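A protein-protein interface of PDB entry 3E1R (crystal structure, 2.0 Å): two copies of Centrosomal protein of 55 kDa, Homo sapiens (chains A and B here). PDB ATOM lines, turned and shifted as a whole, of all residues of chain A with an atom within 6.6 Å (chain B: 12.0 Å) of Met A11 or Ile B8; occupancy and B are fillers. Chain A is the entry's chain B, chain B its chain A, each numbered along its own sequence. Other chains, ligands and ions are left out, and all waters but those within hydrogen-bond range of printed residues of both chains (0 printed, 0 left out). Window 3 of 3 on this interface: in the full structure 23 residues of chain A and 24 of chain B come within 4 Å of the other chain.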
ATOM      1  N   ILE A   8     -23.079  21.330 -26.816  1.00  0.00           N
ATOM      2  CA  ILE A   8     -24.425  20.907 -26.332  1.00  0.00           C
ATOM      3  C   ILE A   8     -25.244  22.170 -26.049  1.00  0.00           C
ATOM      4  O   ILE A   8     -24.701  23.276 -26.055  1.00  0.00           O
ATOM      5  CB  ILE A   8     -24.298  20.040 -25.046  1.00  0.00           C
ATOM      6  CG1 ILE A   8     -25.554  19.189 -24.854  1.00  0.00           C
ATOM      7  CG2 ILE A   8     -24.049  20.923 -23.837  1.00  0.00           C
ATOM      8  CD1 ILE A   8     -25.672  18.028 -25.832  1.00  0.00           C
ATOM      9  N   HIS A   9     -26.542  22.016 -25.803  1.00  0.00           N
ATOM     10  CA  HIS A   9     -27.391  23.176 -25.548  1.00  0.00           C
ATOM     11  C   HIS A   9     -27.827  23.324 -24.092  1.00  0.00           C
ATOM     12  O   HIS A   9     -28.464  24.315 -23.732  1.00  0.00           O
ATOM     13  CB  HIS A   9     -28.632  23.139 -26.445  1.00  0.00           C
ATOM     14  CG  HIS A   9     -29.361  24.445 -26.521  1.00  0.00           C
ATOM     15  ND1 HIS A   9     -30.730  24.528 -26.654  1.00  0.00           N
ATOM     16  CD2 HIS A   9     -28.910  25.722 -26.501  1.00  0.00           C
ATOM     17  CE1 HIS A   9     -31.090  25.798 -26.708  1.00  0.00           C
ATOM     18  NE2 HIS A   9     -30.005  26.543 -26.617  1.00  0.00           N
ATOM     19  N   GLU A  10     -27.505  22.343 -23.252  1.00  0.00           N
ATOM     20  CA  GLU A  10     -27.877  22.441 -21.847  1.00  0.00           C
ATOM     21  C   GLU A  10     -26.873  23.357 -21.166  1.00  0.00           C
ATOM     22  O   GLU A  10     -27.192  24.032 -20.186  1.00  0.00           O
ATOM     23  CB  GLU A  10     -27.882  21.063 -21.170  1.00  0.00           C
ATOM     24  CG  GLU A  10     -26.539  20.346 -21.129  1.00  0.00           C
ATOM     25  CD  GLU A  10     -26.621  19.007 -20.408  1.00  0.00           C
ATOM     26  OE1 GLU A  10     -27.595  18.262 -20.651  1.00  0.00           O
ATOM     27  OE2 GLU A  10     -25.712  18.696 -19.608  1.00  0.00           O
ATOM     28  N   MET A  11     -25.659  23.384 -21.707  1.00  0.00           N
ATOM     29  CA  MET A  11     -24.600  24.216 -21.157  1.00  0.00           C
ATOM     30  C   MET A  11     -24.591  25.594 -21.816  1.00  0.00           C
ATOM     31  O   MET A  11     -23.993  26.532 -21.293  1.00  0.00           O
ATOM     32  CB  MET A  11     -23.239  23.536 -21.330  1.00  0.00           C
ATOM     33  CG  MET A  11     -22.491  23.916 -22.596  1.00  0.00           C
ATOM     34  SD  MET A  11     -20.906  24.682 -22.203  1.00  0.00           S
ATOM     35  CE  MET A  11     -19.875  23.227 -22.052  1.00  0.00           C
ATOM     36  N   GLU A  12     -25.242  25.709 -22.971  1.00  0.00           N
ATOM     37  CA  GLU A  12     -25.316  26.996 -23.654  1.00  0.00           C
ATOM     38  C   GLU A  12     -26.292  27.805 -22.806  1.00  0.00           C
ATOM     39  O   GLU A  12     -26.130  29.010 -22.614  1.00  0.00           O
ATOM     40  CB  GLU A  12     -25.842  26.827 -25.087  1.00  0.00           C
ATOM     41  CG  GLU A  12     -25.417  27.945 -26.041  1.00  0.00           C
ATOM     42  CD  GLU A  12     -25.463  27.530 -27.506  1.00  0.00           C
ATOM     43  OE1 GLU A  12     -24.689  28.101 -28.307  1.00  0.00           O
ATOM     44  OE2 GLU A  12     -26.268  26.643 -27.861  1.00  0.00           O
ATOM     45  N   ILE A  13     -27.301  27.114 -22.285  1.00  0.00           N
ATOM     46  CA  ILE A  13     -28.295  27.734 -21.424  1.00  0.00           C
ATOM     47  C   ILE A  13     -27.603  28.011 -20.087  1.00  0.00           C
ATOM     48  O   ILE A  13     -27.645  29.131 -19.585  1.00  0.00           O
ATOM     49  CB  ILE A  13     -29.529  26.805 -21.214  1.00  0.00           C
ATOM     50  CG1 ILE A  13     -30.374  26.756 -22.494  1.00  0.00           C
ATOM     51  CG2 ILE A  13     -30.355  27.288 -20.027  1.00  0.00           C
ATOM     52  CD1 ILE A  13     -30.945  28.101 -22.938  1.00  0.00           C
ATOM     53  N   GLN A  14     -26.951  26.992 -19.527  1.00  0.00           N
ATOM     54  CA  GLN A  14     -26.241  27.151 -18.255  1.00  0.00           C
ATOM     55  C   GLN A  14     -25.282  28.339 -18.285  1.00  0.00           C
ATOM     56  O   GLN A  14     -25.155  29.060 -17.296  1.00  0.00           O
ATOM     57  CB  GLN A  14     -25.443  25.886 -17.896  1.00  0.00           C
ATOM     58  CG  GLN A  14     -26.236  24.797 -17.184  1.00  0.00           C
ATOM     59  CD  GLN A  14     -25.363  23.636 -16.716  1.00  0.00           C
ATOM     60  OE1 GLN A  14     -25.740  22.472 -16.853  1.00  0.00           O
ATOM     61  NE2 GLN A  14     -24.201  23.951 -16.149  1.00  0.00           N
ATOM     62  N   LEU A  15     -24.613  28.545 -19.417  1.00  0.00           N
ATOM     63  CA  LEU A  15     -23.661  29.647 -19.540  1.00  0.00           C
ATOM     64  C   LEU A  15     -24.289  31.034 -19.472  1.00  0.00           C
ATOM     65  O   LEU A  15     -23.828  31.874 -18.695  1.00  0.00           O
ATOM     66  CB  LEU A  15     -22.843  29.536 -20.832  1.00  0.00           C
ATOM     67  CG  LEU A  15     -21.853  30.688 -21.077  1.00  0.00           C
ATOM     68  CD1 LEU A  15     -20.829  30.743 -19.949  1.00  0.00           C
ATOM     69  CD2 LEU A  15     -21.151  30.500 -22.415  1.00  0.00           C
ATOM     70  N   LYS A  16     -25.317  31.307 -20.270  1.00  0.00           N
ATOM     71  CA  LYS A  16     -25.895  32.641 -20.183  1.00  0.00           C
ATOM     72  C   LYS A  16     -26.651  32.794 -18.876  1.00  0.00           C
ATOM     73  O   LYS A  16     -26.841  33.905 -18.390  1.00  0.00           O
ATOM     74  CB  LYS A  16     -26.823  32.971 -21.352  1.00  0.00           C
ATOM     75  CG  LYS A  16     -26.674  34.437 -21.800  1.00  0.00           C
ATOM     76  CD  LYS A  16     -26.613  35.419 -20.610  1.00  0.00           C
ATOM     77  CE  LYS A  16     -25.694  36.611 -20.893  1.00  0.00           C
ATOM     78  NZ  LYS A  16     -25.608  37.586 -19.759  1.00  0.00           N
ATOM     79  N   ASN B   6     -11.368  24.202 -29.884  1.00  0.00           N
ATOM     80  CA  ASN B   6     -12.778  23.760 -29.697  1.00  0.00           C
ATOM     81  C   ASN B   6     -13.652  24.890 -29.163  1.00  0.00           C
ATOM     82  O   ASN B   6     -13.205  25.705 -28.354  1.00  0.00           O
ATOM     83  CB  ASN B   6     -12.836  22.578 -28.727  1.00  0.00           C
ATOM     84  CG  ASN B   6     -13.377  21.319 -29.373  1.00  0.00           C
ATOM     85  OD1 ASN B   6     -14.513  21.287 -29.845  1.00  0.00           O
ATOM     86  ND2 ASN B   6     -12.564  20.268 -29.395  1.00  0.00           N
ATOM     87  N   ASN B   7     -14.897  24.930 -29.628  1.00  0.00           N
ATOM     88  CA  ASN B   7     -15.855  25.936 -29.184  1.00  0.00           C
ATOM     89  C   ASN B   7     -16.487  25.411 -27.899  1.00  0.00           C
ATOM     90  O   ASN B   7     -16.812  26.175 -26.992  1.00  0.00           O
ATOM     91  CB  ASN B   7     -16.943  26.152 -30.243  1.00  0.00           C
ATOM     92  CG  ASN B   7     -16.399  26.734 -31.538  1.00  0.00           C
ATOM     93  OD1 ASN B   7     -15.544  26.139 -32.193  1.00  0.00           O
ATOM     94  ND2 ASN B   7     -16.903  27.904 -31.913  1.00  0.00           N
ATOM     95  N   ILE B   8     -16.651  24.093 -27.837  1.00  0.00           N
ATOM     96  CA  ILE B   8     -17.237  23.438 -26.673  1.00  0.00           C
ATOM     97  C   ILE B   8     -16.383  23.650 -25.425  1.00  0.00           C
ATOM     98  O   ILE B   8     -16.908  23.840 -24.330  1.00  0.00           O
ATOM     99  CB  ILE B   8     -17.399  21.915 -26.901  1.00  0.00           C
ATOM    100  CG1 ILE B   8     -16.059  21.300 -27.310  1.00  0.00           C
ATOM    101  CG2 ILE B   8     -18.462  21.656 -27.960  1.00  0.00           C
ATOM    102  CD1 ILE B   8     -16.017  19.784 -27.234  1.00  0.00           C
ATOM    103  N   HIS B   9     -15.065  23.614 -25.593  1.00  0.00           N
ATOM    104  CA  HIS B   9     -14.162  23.806 -24.466  1.00  0.00           C
ATOM    105  C   HIS B   9     -14.124  25.267 -24.039  1.00  0.00           C
ATOM    106  O   HIS B   9     -14.041  25.569 -22.848  1.00  0.00           O
ATOM    107  CB  HIS B   9     -12.749  23.325 -24.823  1.00  0.00           C
ATOM    108  CG  HIS B   9     -12.631  21.837 -24.966  1.00  0.00           C
ATOM    109  ND1 HIS B   9     -11.455  21.215 -25.324  1.00  0.00           N
ATOM    110  CD2 HIS B   9     -13.541  20.848 -24.791  1.00  0.00           C
ATOM    111  CE1 HIS B   9     -11.643  19.908 -25.364  1.00  0.00           C
ATOM    112  NE2 HIS B   9     -12.900  19.659 -25.043  1.00  0.00           N
ATOM    113  N   GLU B  10     -14.190  26.175 -25.009  1.00  0.00           N
ATOM    114  CA  GLU B  10     -14.160  27.602 -24.709  1.00  0.00           C
ATOM    115  C   GLU B  10     -15.404  28.025 -23.933  1.00  0.00           C
ATOM    116  O   GLU B  10     -15.346  28.949 -23.125  1.00  0.00           O
ATOM    117  CB  GLU B  10     -14.037  28.420 -26.000  1.00  0.00           C
ATOM    118  CG  GLU B  10     -14.059  29.940 -25.804  1.00  0.00           C
ATOM    119  CD  GLU B  10     -12.912  30.462 -24.953  1.00  0.00           C
ATOM    120  OE1 GLU B  10     -12.814  31.698 -24.780  1.00  0.00           O
ATOM    121  OE2 GLU B  10     -12.104  29.647 -24.455  1.00  0.00           O
ATOM    122  N   MET B  11     -16.523  27.349 -24.176  1.00  0.00           N
ATOM    123  CA  MET B  11     -17.771  27.662 -23.483  1.00  0.00           C
ATOM    124  C   MET B  11     -17.789  27.112 -22.054  1.00  0.00           C
ATOM    125  O   MET B  11     -18.335  27.743 -21.149  1.00  0.00           O
ATOM    126  CB  MET B  11     -18.974  27.100 -24.250  1.00  0.00           C
ATOM    127  CG  MET B  11     -19.603  28.050 -25.267  1.00  0.00           C
ATOM    128  SD  MET B  11     -21.082  27.330 -26.045  1.00  0.00           S
ATOM    129  CE  MET B  11     -22.093  27.018 -24.616  1.00  0.00           C
ATOM    130  N   GLU B  12     -17.190  25.940 -21.853  1.00  0.00           N
ATOM    131  CA  GLU B  12     -17.164  25.309 -20.534  1.00  0.00           C
ATOM    132  C   GLU B  12     -16.178  25.980 -19.550  1.00  0.00           C
ATOM    133  O   GLU B  12     -16.457  26.074 -18.359  1.00  0.00           O
ATOM    134  CB  GLU B  12     -16.861  23.804 -20.694  1.00  0.00           C
ATOM    135  CG  GLU B  12     -17.496  22.898 -19.625  1.00  0.00           C
ATOM    136  CD  GLU B  12     -17.560  21.426 -20.035  1.00  0.00           C
ATOM    137  OE1 GLU B  12     -17.225  21.107 -21.198  1.00  0.00           O
ATOM    138  OE2 GLU B  12     -17.955  20.585 -19.195  1.00  0.00           O
ATOM    139  N   ILE B  13     -15.036  26.447 -20.060  1.00  0.00           N
ATOM    140  CA  ILE B  13     -13.987  27.128 -19.272  1.00  0.00           C
ATOM    141  C   ILE B  13     -14.592  28.401 -18.695  1.00  0.00           C
ATOM    142  O   ILE B  13     -14.292  28.900 -17.606  1.00  0.00           O
ATOM    143  CB  ILE B  13     -12.844  27.566 -20.223  1.00  0.00           C
ATOM    144  CG1 ILE B  13     -12.008  26.358 -20.627  1.00  0.00           C
ATOM    145  CG2 ILE B  13     -12.043  28.691 -19.596  1.00  0.00           C
ATOM    146  CD1 ILE B  13     -11.067  26.641 -21.792  1.00  0.00           C
ATOM    147  N   GLN B  14     -15.440  28.893 -19.566  1.00  0.00           N
ATOM    148  CA  GLN B  14     -16.250  30.083 -19.547  1.00  0.00           C
ATOM    149  C   GLN B  14     -17.370  30.001 -18.497  1.00  0.00           C
ATOM    150  O   GLN B  14     -17.635  30.960 -17.756  1.00  0.00           O
ATOM    151  CB  GLN B  14     -16.790  30.101 -20.962  1.00  0.00           C
ATOM    152  CG  GLN B  14     -17.647  31.192 -21.387  1.00  0.00           C
ATOM    153  CD  GLN B  14     -16.885  32.455 -21.563  1.00  0.00           C
ATOM    154  OE1 GLN B  14     -15.662  32.449 -21.720  1.00  0.00           O
ATOM    155  NE2 GLN B  14     -17.601  33.565 -21.543  1.00  0.00           N
ATOM    156  N   LEU B  15     -18.024  28.846 -18.470  1.00  0.00           N
ATOM    157  CA  LEU B  15     -19.101  28.561 -17.540  1.00  0.00           C
ATOM    158  C   LEU B  15     -18.485  28.389 -16.158  1.00  0.00           C
ATOM    159  O   LEU B  15     -18.988  28.925 -15.174  1.00  0.00           O
ATOM    160  CB  LEU B  15     -19.811  27.278 -17.978  1.00  0.00           C
ATOM    161  CG  LEU B  15     -20.901  26.681 -17.085  1.00  0.00           C
ATOM    162  CD1 LEU B  15     -21.993  27.707 -16.831  1.00  0.00           C
ATOM    163  CD2 LEU B  15     -21.475  25.446 -17.759  1.00  0.00           C
ATOM    164  N   LYS B  16     -17.392  27.637 -16.094  1.00  0.00           N
ATOM    165  CA  LYS B  16     -16.712  27.411 -14.825  1.00  0.00           C
ATOM    166  C   LYS B  16     -16.262  28.730 -14.191  1.00  0.00           C
ATOM    167  O   LYS B  16     -16.358  28.903 -12.978  1.00  0.00           O
ATOM    168  CB  LYS B  16     -15.497  26.494 -15.011  1.00  0.00           C
ATOM    169  CG  LYS B  16     -15.760  25.007 -14.749  1.00  0.00           C
ATOM    170  CD  LYS B  16     -16.502  24.336 -15.894  1.00  0.00           C
ATOM    171  CE  LYS B  16     -16.457  22.812 -15.781  1.00  0.00           C
ATOM    172  NZ  LYS B  16     -17.150  22.289 -14.571  1.00  0.00           N
ATOM    173  N   ASP B  17     -15.775  29.661 -15.008  1.00  0.00           N
ATOM    174  CA  ASP B  17     -15.329  30.956 -14.497  1.00  0.00           C
ATOM    175  C   ASP B  17     -16.512  31.723 -13.905  1.00  0.00           C
ATOM    176  O   ASP B  17     -16.442  32.228 -12.782  1.00  0.00           O
ATOM    177  CB  ASP B  17     -14.684  31.782 -15.615  1.00  0.00           C
ATOM    178  CG  ASP B  17     -14.264  33.169 -15.149  1.00  0.00           C
ATOM    179  OD1 ASP B  17     -13.421  33.266 -14.232  1.00  0.00           O
ATOM    180  OD2 ASP B  17     -14.776  34.163 -15.705  1.00  0.00           O
ATOM    181  N   ALA B  18     -17.600  31.795 -14.665  1.00  0.00           N
ATOM    182  CA  ALA B  18     -18.801  32.500 -14.231  1.00  0.00           C
ATOM    183  C   ALA B  18     -19.409  31.905 -12.968  1.00  0.00           C
ATOM    184  O   ALA B  18     -19.823  32.637 -12.069  1.00  0.00           O
ATOM    185  CB  ALA B  18     -19.835  32.503 -15.347  1.00  0.00           C
ATOM    186  N   LEU B  19     -19.483  30.579 -12.907  1.00  0.00           N
ATOM    187  CA  LEU B  19     -20.047  29.917 -11.739  1.00  0.00           C
ATOM    188  C   LEU B  19     -19.213  30.246 -10.516  1.00  0.00           C
ATOM    189  O   LEU B  19     -19.742  30.546  -9.452  1.00  0.00           O
ATOM    190  CB  LEU B  19     -20.092  28.401 -11.946  1.00  0.00           C
ATOM    191  CG  LEU B  19     -21.017  27.918 -13.068  1.00  0.00           C
ATOM    192  CD1 LEU B  19     -20.925  26.403 -13.195  1.00  0.00           C
ATOM    193  CD2 LEU B  19     -22.448  28.350 -12.771  1.00  0.00           C
ATOM    194  N   ASN B  22     -19.865  33.839  -9.442  1.00  0.00           N
ATOM    195  CA  ASN B  22     -21.175  34.019  -8.819  1.00  0.00           C
ATOM    196  C   ASN B  22     -21.178  33.441  -7.405  1.00  0.00           C
ATOM    197  O   ASN B  22     -21.830  33.981  -6.517  1.00  0.00           O
ATOM    198  CB  ASN B  22     -22.282  33.359  -9.649  1.00  0.00           C
ATOM    199  CG  ASN B  22     -22.547  34.087 -10.953  1.00  0.00           C
ATOM    200  OD1 ASN B  22     -22.139  35.234 -11.127  1.00  0.00           O
ATOM    201  ND2 ASN B  22     -23.250  33.425 -11.868  1.00  0.00           N
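Met A11 touches Ile B8 (CE to O, 3.8 Å). Met A11 touches Met B11 (SD to CE, 3.6 Å). Met A11 touches Glu B12 (CE to CB, 3.4 Å). Met B11 touches Glu A12. Gln A14 touches Leu B15. CD1 of Leu A15 touches CG of Gln B14, 3.5 Å away. CD1 of Leu A15 touches CA of Leu B15, at 3.7 Å.
No residue of chain B comes within 4 Å of Ile A8. His A9 touches none of the printed residues of chain B. No residue of chain B comes within 4 Å of Glu A10. Met A11 touches three residues of chain B. Gln A14 touches just one residue of chain B: Leu B15. Of the printed residues of chain A, Met B11 touches Met A11 (3.6 Å) and Glu A12 (3.4 Å). Printed residues of chain A within 4 Å of Glu B12: Met A11. Of the printed residues of chain A, Gln B14 touches Leu A15 (3.5 Å). Of the printed residues of chain A, Leu B15 touches Gln A14 and Leu A15. The nearest residue of chain B that does not touch Met A11 is Leu B15 (4.4 Å). The nearest residue of chain A that does not touch Ile B8 is Ile A8 (4.8 Å). The nearest printed residue of chain A that does not touch Gln B14 is Met A11 (6.9 Å).
Hydrophobic or aromatic side chains of chain A within 4 Å of the printed part of chain B: Met A11 and Leu A15. Of the 15 printed residues of chain B, 5 touch a printed residue of chain A. Hydrophobic or aromatic side chains of chain B within 4 Å of the printed part of chain A: Met B11 and Leu B15. Among the printed residues, 7 pairs touch across the chains.
Met A11 touches Ile B8, but with the chains exchanged Ile A8 does not touch Met B11 (4.8 Å). Met B11 touches its own counterpart, Met A11. Met A11 touches Glu B12, and with the chains exchanged Glu A12 touches Met B11. Gln A14 touches Leu B15, and with the chains exchanged Leu A15 touches Gln B14.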
